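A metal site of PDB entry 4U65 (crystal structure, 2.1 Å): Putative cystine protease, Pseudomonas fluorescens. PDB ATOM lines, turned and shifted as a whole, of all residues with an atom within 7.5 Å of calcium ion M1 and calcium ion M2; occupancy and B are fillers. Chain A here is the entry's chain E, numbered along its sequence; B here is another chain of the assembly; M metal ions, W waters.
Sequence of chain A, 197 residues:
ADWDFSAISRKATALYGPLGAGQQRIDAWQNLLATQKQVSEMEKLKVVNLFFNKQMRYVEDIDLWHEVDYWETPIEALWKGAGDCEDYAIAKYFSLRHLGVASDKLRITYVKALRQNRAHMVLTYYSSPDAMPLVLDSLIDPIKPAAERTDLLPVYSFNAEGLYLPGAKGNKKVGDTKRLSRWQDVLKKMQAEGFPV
The indole nitrogen of Trp 71 is in hydrogen-bond range of the side-chain carboxylate of Asp 69 (3.3 Å).
OD2 of Asp 69 lies within salt-bridge range of NH2 of Arg 182 (3.8 Å).
SG of Cys 85 lies close to OE2 of Glu 86 (3.5 Å).
OD1 of Asp 87 lies close to N of Glu 72, at 2.8 Å.
Five residues have an atom within 4 Å of calcium ion M2: Asp 61, Tyr 70, Asp 84, Glu 86 and Asp 87.
Four residues have an atom within 4 Å of calcium ion M1: Asp 61, Asp 69, Asp 84 and Glu 86.
Along chain A the residues within 4 Å of calcium ion M1 span positions 61 to 86.
The nearest printed residue that does not touch calcium ion M1 is Tyr 70 (4.3 Å).
Calcium ion M2 is bound by O of Tyr 70, 2.3 Å away.
Calcium ion M2 is bound by OD1 of Asp 84.
OE1 of Glu 86 is bound to calcium ion M2, 2.4 Å away.
OD2 of Asp 87 is bound to calcium ion M2, at 2.4 Å.
OD1 of Asp 61 is bound to calcium ion M2 (2.5 Å).
Calcium ion M2 is bound by the side-chain carboxylate (OD1) of Asp 87.
Calcium ion M2 is bound by OD2 of Asp 61 (2.7 Å).
Calcium ion M2 has seven donor atoms within binding distance.
Calcium ion M1 is bound by the side-chain carboxylate (OD1) of Asp 69 (2.4 Å), the side-chain carboxylate (OD2) of Asp 84 (2.4 Å), the side-chain carboxylate (OD2) of Asp 61 (2.5 Å), the side-chain carboxylate (OE1) of Glu 86 (2.5 Å), water W2 (2.5 Å), the side-chain carboxylate (OE2) of Glu 86 (2.5 Å) and water W1 (2.7 Å).
Calcium ion M1 has seven donor atoms within binding distance.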
ATOM      1  N   TYR A  58     -36.166 -14.817  -7.275  1.00  0.00           N
ATOM      2  CA  TYR A  58     -35.941 -15.536  -6.022  1.00  0.00           C
ATOM      3  C   TYR A  58     -36.129 -17.030  -6.267  1.00  0.00           C
ATOM      4  O   TYR A  58     -37.232 -17.481  -6.576  1.00  0.00           O
ATOM      5  CB  TYR A  58     -36.885 -15.039  -4.927  1.00  0.00           C
ATOM      6  CG  TYR A  58     -36.428 -15.428  -3.540  1.00  0.00           C
ATOM      7  CD1 TYR A  58     -36.560 -16.734  -3.072  1.00  0.00           C
ATOM      8  CD2 TYR A  58     -35.862 -14.479  -2.689  1.00  0.00           C
ATOM      9  CE1 TYR A  58     -36.133 -17.082  -1.797  1.00  0.00           C
ATOM     10  CE2 TYR A  58     -35.444 -14.822  -1.416  1.00  0.00           C
ATOM     11  CZ  TYR A  58     -35.579 -16.126  -0.981  1.00  0.00           C
ATOM     12  OH  TYR A  58     -35.165 -16.478   0.289  1.00  0.00           O
ATOM     13  N   VAL A  59     -35.046 -17.796  -6.133  1.00  0.00           N
ATOM     14  CA  VAL A  59     -35.100 -19.251  -6.208  1.00  0.00           C
ATOM     15  C   VAL A  59     -34.199 -19.830  -5.134  1.00  0.00           C
ATOM     16  O   VAL A  59     -33.131 -19.285  -4.844  1.00  0.00           O
ATOM     17  CB  VAL A  59     -34.737 -19.781  -7.620  1.00  0.00           C
ATOM     18  CG1 VAL A  59     -34.387 -18.638  -8.562  1.00  0.00           C
ATOM     19  CG2 VAL A  59     -33.618 -20.807  -7.568  1.00  0.00           C
ATOM     20  N   GLU A  60     -34.653 -20.908  -4.508  1.00  0.00           N
ATOM     21  CA  GLU A  60     -33.924 -21.519  -3.393  1.00  0.00           C
ATOM     22  C   GLU A  60     -32.595 -22.100  -3.872  1.00  0.00           C
ATOM     23  O   GLU A  60     -32.436 -22.482  -5.033  1.00  0.00           O
ATOM     24  CB  GLU A  60     -34.775 -22.614  -2.749  1.00  0.00           C
ATOM     25  CG  GLU A  60     -36.178 -22.179  -2.318  1.00  0.00           C
ATOM     26  CD  GLU A  60     -36.163 -21.143  -1.208  1.00  0.00           C
ATOM     27  OE1 GLU A  60     -35.165 -21.078  -0.460  1.00  0.00           O
ATOM     28  OE2 GLU A  60     -37.159 -20.392  -1.078  1.00  0.00           O
ATOM     29  N   ASP A  61     -31.638 -22.167  -2.945  1.00  0.00           N
ATOM     30  CA  ASP A  61     -30.298 -22.632  -3.295  1.00  0.00           C
ATOM     31  C   ASP A  61     -30.309 -24.084  -3.761  1.00  0.00           C
ATOM     32  O   ASP A  61     -29.539 -24.459  -4.641  1.00  0.00           O
ATOM     33  CB  ASP A  61     -29.352 -22.479  -2.102  1.00  0.00           C
ATOM     34  CG  ASP A  61     -28.928 -21.039  -1.878  1.00  0.00           C
ATOM     35  OD1 ASP A  61     -29.045 -20.228  -2.833  1.00  0.00           O
ATOM     36  OD2 ASP A  61     -28.468 -20.718  -0.766  1.00  0.00           O
ATOM     37  N   ILE A  62     -31.186 -24.910  -3.181  1.00  0.00           N
ATOM     38  CA  ILE A  62     -31.225 -26.324  -3.544  1.00  0.00           C
ATOM     39  C   ILE A  62     -31.629 -26.507  -5.012  1.00  0.00           C
ATOM     40  O   ILE A  62     -31.239 -27.481  -5.658  1.00  0.00           O
ATOM     41  CB  ILE A  62     -32.161 -27.105  -2.591  1.00  0.00           C
ATOM     42  CG1 ILE A  62     -32.049 -28.612  -2.830  1.00  0.00           C
ATOM     43  CG2 ILE A  62     -33.610 -26.647  -2.752  1.00  0.00           C
ATOM     44  CD1 ILE A  62     -30.673 -29.173  -2.529  1.00  0.00           C
ATOM     45  N   LEU A  64     -31.218 -23.893  -7.514  1.00  0.00           N
ATOM     46  CA  LEU A  64     -30.298 -23.193  -8.409  1.00  0.00           C
ATOM     47  C   LEU A  64     -28.885 -23.775  -8.345  1.00  0.00           C
ATOM     48  O   LEU A  64     -28.199 -23.872  -9.372  1.00  0.00           O
ATOM     49  CB  LEU A  64     -30.266 -21.699  -8.068  1.00  0.00           C
ATOM     50  CG  LEU A  64     -29.485 -20.774  -9.010  1.00  0.00           C
ATOM     51  CD1 LEU A  64     -29.941 -20.951 -10.452  1.00  0.00           C
ATOM     52  CD2 LEU A  64     -29.628 -19.330  -8.567  1.00  0.00           C
ATOM     53  N   TRP A  65     -28.441 -24.173  -7.157  1.00  0.00           N
ATOM     54  CA  TRP A  65     -27.078 -24.637  -6.952  1.00  0.00           C
ATOM     55  C   TRP A  65     -26.994 -26.110  -6.552  1.00  0.00           C
ATOM     56  O   TRP A  65     -25.886 -26.632  -6.415  1.00  0.00           O
ATOM     57  CB  TRP A  65     -26.391 -23.772  -5.890  1.00  0.00           C
ATOM     58  CG  TRP A  65     -26.356 -22.329  -6.274  1.00  0.00           C
ATOM     59  CD1 TRP A  65     -27.176 -21.343  -5.820  1.00  0.00           C
ATOM     60  CD2 TRP A  65     -25.472 -21.713  -7.216  1.00  0.00           C
ATOM     61  NE1 TRP A  65     -26.859 -20.145  -6.422  1.00  0.00           N
ATOM     62  CE2 TRP A  65     -25.809 -20.355  -7.274  1.00  0.00           C
ATOM     63  CE3 TRP A  65     -24.424 -22.185  -8.014  1.00  0.00           C
ATOM     64  CZ2 TRP A  65     -25.133 -19.452  -8.095  1.00  0.00           C
ATOM     65  CZ3 TRP A  65     -23.747 -21.297  -8.827  1.00  0.00           C
ATOM     66  CH2 TRP A  65     -24.116 -19.942  -8.863  1.00  0.00           C
ATOM     67  N   GLU A  67     -27.487 -27.247  -3.763  1.00  0.00           N
ATOM     68  CA  GLU A  67     -26.889 -27.199  -2.430  1.00  0.00           C
ATOM     69  C   GLU A  67     -27.873 -26.521  -1.503  1.00  0.00           C
ATOM     70  O   GLU A  67     -28.529 -25.547  -1.893  1.00  0.00           O
ATOM     71  CB  GLU A  67     -25.552 -26.447  -2.431  1.00  0.00           C
ATOM     72  CG  GLU A  67     -24.439 -27.153  -3.188  1.00  0.00           C
ATOM     73  CD  GLU A  67     -23.951 -28.387  -2.469  1.00  0.00           C
ATOM     74  OE1 GLU A  67     -24.227 -28.501  -1.255  1.00  0.00           O
ATOM     75  OE2 GLU A  67     -23.314 -29.243  -3.107  1.00  0.00           O
ATOM     76  N   VAL A  68     -27.987 -27.038  -0.274  1.00  0.00           N
ATOM     77  CA  VAL A  68     -28.948 -26.473   0.676  1.00  0.00           C
ATOM     78  C   VAL A  68     -28.644 -25.003   0.926  1.00  0.00           C
ATOM     79  O   VAL A  68     -29.562 -24.166   0.958  1.00  0.00           O
ATOM     80  CB  VAL A  68     -28.922 -27.284   1.984  1.00  0.00           C
ATOM     81  CG1 VAL A  68     -29.721 -26.566   3.068  1.00  0.00           C
ATOM     82  CG2 VAL A  68     -29.479 -28.675   1.742  1.00  0.00           C
ATOM     83  N   ASP A  69     -27.374 -24.657   1.085  1.00  0.00           N
ATOM     84  CA  ASP A  69     -26.975 -23.267   1.292  1.00  0.00           C
ATOM     85  C   ASP A  69     -25.769 -22.963   0.414  1.00  0.00           C
ATOM     86  O   ASP A  69     -24.787 -23.717   0.418  1.00  0.00           O
ATOM     87  CB  ASP A  69     -26.636 -23.009   2.770  1.00  0.00           C
ATOM     88  CG  ASP A  69     -26.808 -21.557   3.161  1.00  0.00           C
ATOM     89  OD1 ASP A  69     -27.515 -20.833   2.446  1.00  0.00           O
ATOM     90  OD2 ASP A  69     -26.229 -21.151   4.189  1.00  0.00           O
ATOM     91  N   TYR A  70     -25.855 -21.872  -0.346  1.00  0.00           N
ATOM     92  CA  TYR A  70     -24.771 -21.485  -1.254  1.00  0.00           C
ATOM     93  C   TYR A  70     -24.803 -19.965  -1.382  1.00  0.00           C
ATOM     94  O   TYR A  70     -25.750 -19.410  -1.929  1.00  0.00           O
ATOM     95  CB  TYR A  70     -24.915 -22.149  -2.619  1.00  0.00           C
ATOM     96  CG  TYR A  70     -23.763 -21.865  -3.562  1.00  0.00           C
ATOM     97  CD1 TYR A  70     -23.787 -20.766  -4.406  1.00  0.00           C
ATOM     98  CD2 TYR A  70     -22.654 -22.704  -3.602  1.00  0.00           C
ATOM     99  CE1 TYR A  70     -22.730 -20.500  -5.257  1.00  0.00           C
ATOM    100  CE2 TYR A  70     -21.601 -22.447  -4.455  1.00  0.00           C
ATOM    101  CZ  TYR A  70     -21.639 -21.345  -5.283  1.00  0.00           C
ATOM    102  OH  TYR A  70     -20.590 -21.090  -6.127  1.00  0.00           O
ATOM    103  N   TRP A  71     -23.758 -19.304  -0.878  1.00  0.00           N
ATOM    104  CA  TRP A  71     -23.701 -17.838  -0.876  1.00  0.00           C
ATOM    105  C   TRP A  71     -23.087 -17.358  -2.192  1.00  0.00           C
ATOM    106  O   TRP A  71     -21.913 -17.604  -2.460  1.00  0.00           O
ATOM    107  CB  TRP A  71     -22.904 -17.330   0.320  1.00  0.00           C
ATOM    108  CG  TRP A  71     -23.609 -17.520   1.639  1.00  0.00           C
ATOM    109  CD1 TRP A  71     -24.602 -18.411   1.921  1.00  0.00           C
ATOM    110  CD2 TRP A  71     -23.385 -16.772   2.842  1.00  0.00           C
ATOM    111  NE1 TRP A  71     -25.002 -18.271   3.228  1.00  0.00           N
ATOM    112  CE2 TRP A  71     -24.279 -17.275   3.809  1.00  0.00           C
ATOM    113  CE3 TRP A  71     -22.518 -15.736   3.191  1.00  0.00           C
ATOM    114  CZ2 TRP A  71     -24.324 -16.776   5.114  1.00  0.00           C
ATOM    115  CZ3 TRP A  71     -22.568 -15.231   4.484  1.00  0.00           C
ATOM    116  CH2 TRP A  71     -23.456 -15.753   5.430  1.00  0.00           C
ATOM    117  N   GLU A  72     -23.888 -16.673  -3.000  1.00  0.00           N
ATOM    118  CA  GLU A  72     -23.448 -16.173  -4.289  1.00  0.00           C
ATOM    119  C   GLU A  72     -22.595 -14.924  -4.137  1.00  0.00           C
ATOM    120  O   GLU A  72     -22.868 -14.065  -3.285  1.00  0.00           O
ATOM    121  CB  GLU A  72     -24.648 -15.834  -5.174  1.00  0.00           C
ATOM    122  CG  GLU A  72     -25.495 -17.008  -5.591  1.00  0.00           C
ATOM    123  CD  GLU A  72     -26.752 -16.575  -6.320  1.00  0.00           C
ATOM    124  OE1 GLU A  72     -27.111 -15.380  -6.207  1.00  0.00           O
ATOM    125  OE2 GLU A  72     -27.369 -17.416  -7.001  1.00  0.00           O
ATOM    126  N   ALA A  82     -30.474 -14.846 -10.503  1.00  0.00           N
ATOM    127  CA  ALA A  82     -31.314 -15.517  -9.532  1.00  0.00           C
ATOM    128  C   ALA A  82     -30.508 -15.817  -8.276  1.00  0.00           C
ATOM    129  O   ALA A  82     -29.281 -15.910  -8.309  1.00  0.00           O
ATOM    130  CB  ALA A  82     -31.900 -16.805 -10.111  1.00  0.00           C
ATOM    131  N   GLY A  83     -31.224 -15.976  -7.171  1.00  0.00           N
ATOM    132  CA  GLY A  83     -30.605 -16.259  -5.893  1.00  0.00           C
ATOM    133  C   GLY A  83     -31.662 -16.278  -4.800  1.00  0.00           C
ATOM    134  O   GLY A  83     -32.853 -16.136  -5.070  1.00  0.00           O
ATOM    135  N   ASP A  84     -31.191 -16.448  -3.568  1.00  0.00           N
ATOM    136  CA  ASP A  84     -32.110 -16.419  -2.440  1.00  0.00           C
ATOM    137  C   ASP A  84     -31.742 -15.306  -1.462  1.00  0.00           C
ATOM    138  O   ASP A  84     -31.027 -14.377  -1.826  1.00  0.00           O
ATOM    139  CB  ASP A  84     -32.172 -17.788  -1.743  1.00  0.00           C
ATOM    140  CG  ASP A  84     -30.930 -18.111  -0.938  1.00  0.00           C
ATOM    141  OD1 ASP A  84     -29.887 -17.454  -1.121  1.00  0.00           O
ATOM    142  OD2 ASP A  84     -31.002 -19.032  -0.099  1.00  0.00           O
ATOM    143  N   CYS A  85     -32.199 -15.425  -0.206  1.00  0.00           N
ATOM    144  CA  CYS A  85     -32.253 -14.272   0.695  1.00  0.00           C
ATOM    145  C   CYS A  85     -30.873 -13.644   0.893  1.00  0.00           C
ATOM    146  O   CYS A  85     -30.722 -12.422   0.751  1.00  0.00           O
ATOM    147  CB  CYS A  85     -32.857 -14.684   2.036  1.00  0.00           C
ATOM    148  SG  CYS A  85     -32.016 -16.025   2.895  1.00  0.00           S
ATOM    149  N   GLU A  86     -29.863 -14.449   1.220  1.00  0.00           N
ATOM    150  CA  GLU A  86     -28.554 -13.860   1.506  1.00  0.00           C
ATOM    151  C   GLU A  86     -27.870 -13.362   0.238  1.00  0.00           C
ATOM    152  O   GLU A  86     -27.077 -12.415   0.301  1.00  0.00           O
ATOM    153  CB  GLU A  86     -27.652 -14.851   2.237  1.00  0.00           C
ATOM    154  CG  GLU A  86     -27.002 -15.906   1.369  1.00  0.00           C
ATOM    155  CD  GLU A  86     -27.815 -17.176   1.292  1.00  0.00           C
ATOM    156  OE1 GLU A  86     -27.415 -18.083   0.531  1.00  0.00           O
ATOM    157  OE2 GLU A  86     -28.854 -17.258   1.985  1.00  0.00           O
ATOM    158  N   ASP A  87     -28.171 -13.973  -0.906  1.00  0.00           N
ATOM    159  CA  ASP A  87     -27.568 -13.529  -2.168  1.00  0.00           C
ATOM    160  C   ASP A  87     -27.947 -12.083  -2.462  1.00  0.00           C
ATOM    161  O   ASP A  87     -27.097 -11.276  -2.840  1.00  0.00           O
ATOM    162  CB  ASP A  87     -28.012 -14.442  -3.313  1.00  0.00           C
ATOM    163  CG  ASP A  87     -27.646 -15.889  -3.067  1.00  0.00           C
ATOM    164  OD1 ASP A  87     -26.620 -16.153  -2.393  1.00  0.00           O
ATOM    165  OD2 ASP A  87     -28.385 -16.769  -3.550  1.00  0.00           O
ATOM    166  N   TYR A  88     -29.228 -11.739  -2.292  1.00  0.00           N
ATOM    167  CA  TYR A  88     -29.665 -10.355  -2.455  1.00  0.00           C
ATOM    168  C   TYR A  88     -28.913  -9.428  -1.499  1.00  0.00           C
ATOM    169  O   TYR A  88     -28.411  -8.376  -1.908  1.00  0.00           O
ATOM    170  CB  TYR A  88     -31.168 -10.230  -2.204  1.00  0.00           C
ATOM    171  CG  TYR A  88     -32.078 -10.792  -3.277  1.00  0.00           C
ATOM    172  CD1 TYR A  88     -32.239 -12.163  -3.441  1.00  0.00           C
ATOM    173  CD2 TYR A  88     -32.819  -9.947  -4.093  1.00  0.00           C
ATOM    174  CE1 TYR A  88     -33.090 -12.676  -4.400  1.00  0.00           C
ATOM    175  CE2 TYR A  88     -33.671 -10.446  -5.060  1.00  0.00           C
ATOM    176  CZ  TYR A  88     -33.806 -11.810  -5.214  1.00  0.00           C
ATOM    177  OH  TYR A  88     -34.649 -12.328  -6.170  1.00  0.00           O
ATOM    178  N   ILE A  90     -25.996  -9.829   0.056  1.00  0.00           N
ATOM    179  CA  ILE A  90     -24.570  -9.715  -0.270  1.00  0.00           C
ATOM    180  C   ILE A  90     -24.369  -8.796  -1.470  1.00  0.00           C
ATOM    181  O   ILE A  90     -23.487  -7.930  -1.475  1.00  0.00           O
ATOM    182  CB  ILE A  90     -23.969 -11.110  -0.533  1.00  0.00           C
ATOM    183  CG1 ILE A  90     -23.916 -11.920   0.764  1.00  0.00           C
ATOM    184  CG2 ILE A  90     -22.584 -10.994  -1.152  1.00  0.00           C
ATOM    185  CD1 ILE A  90     -23.614 -13.393   0.555  1.00  0.00           C
ATOM    186  N   MET A 121     -32.847 -13.507   5.674  1.00  0.00           N
ATOM    187  CA  MET A 121     -31.783 -12.543   5.835  1.00  0.00           C
ATOM    188  C   MET A 121     -32.104 -11.271   5.062  1.00  0.00           C
ATOM    189  O   MET A 121     -32.638 -11.333   3.954  1.00  0.00           O
ATOM    190  CB  MET A 121     -30.437 -13.111   5.363  1.00  0.00           C
ATOM    191  CG  MET A 121     -29.286 -12.134   5.493  1.00  0.00           C
ATOM    192  SD  MET A 121     -27.716 -12.801   4.945  1.00  0.00           S
ATOM    193  CE  MET A 121     -27.553 -14.225   6.024  1.00  0.00           C
ATOM    194  N   ARG A 182     -18.368 -18.837   5.724  1.00  0.00           N
ATOM    195  CA  ARG A 182     -19.286 -18.492   4.640  1.00  0.00           C
ATOM    196  C   ARG A 182     -18.894 -17.179   3.965  1.00  0.00           C
ATOM    197  O   ARG A 182     -18.791 -17.102   2.738  1.00  0.00           O
ATOM    198  CB  ARG A 182     -20.716 -18.403   5.168  1.00  0.00           C
ATOM    199  CG  ARG A 182     -21.356 -19.744   5.494  1.00  0.00           C
ATOM    200  CD  ARG A 182     -21.855 -20.454   4.243  1.00  0.00           C
ATOM    201  NE  ARG A 182     -22.461 -21.740   4.568  1.00  0.00           N
ATOM    202  CZ  ARG A 182     -22.949 -22.598   3.673  1.00  0.00           C
ATOM    203  NH1 ARG A 182     -22.890 -22.301   2.379  1.00  0.00           N
ATOM    204  NH2 ARG A 182     -23.477 -23.738   4.070  1.00  0.00           N
ATOM    205  N   LYS B  49     -27.742 -20.824  12.570  1.00  0.00           N
ATOM    206  CA  LYS B  49     -27.138 -20.373  11.321  1.00  0.00           C
ATOM    207  C   LYS B  49     -26.191 -19.211  11.557  1.00  0.00           C
ATOM    208  O   LYS B  49     -25.080 -19.188  10.999  1.00  0.00           O
ATOM    209  CB  LYS B  49     -28.229 -19.980  10.322  1.00  0.00           C
ATOM    210  CG  LYS B  49     -28.484 -20.994   9.228  1.00  0.00           C
ATOM    211  CD  LYS B  49     -29.689 -20.607   8.381  1.00  0.00           C
ATOM    212  CE  LYS B  49     -29.566 -19.176   7.865  1.00  0.00           C
ATOM    213  NZ  LYS B  49     -30.650 -18.813   6.907  1.00  0.00           N
HETATM  214 CA    CA M   1     -29.178 -19.615   1.310  1.00  0.00          CA
HETATM  215 CA    CA M   2     -27.799 -18.328  -1.797  1.00  0.00          CA
HETATM  216  O   HOH W   1     -30.877 -18.891   3.214  1.00  0.00           O
HETATM  217  O   HOH W   2     -30.472 -21.638   1.868  1.00  0.00           O
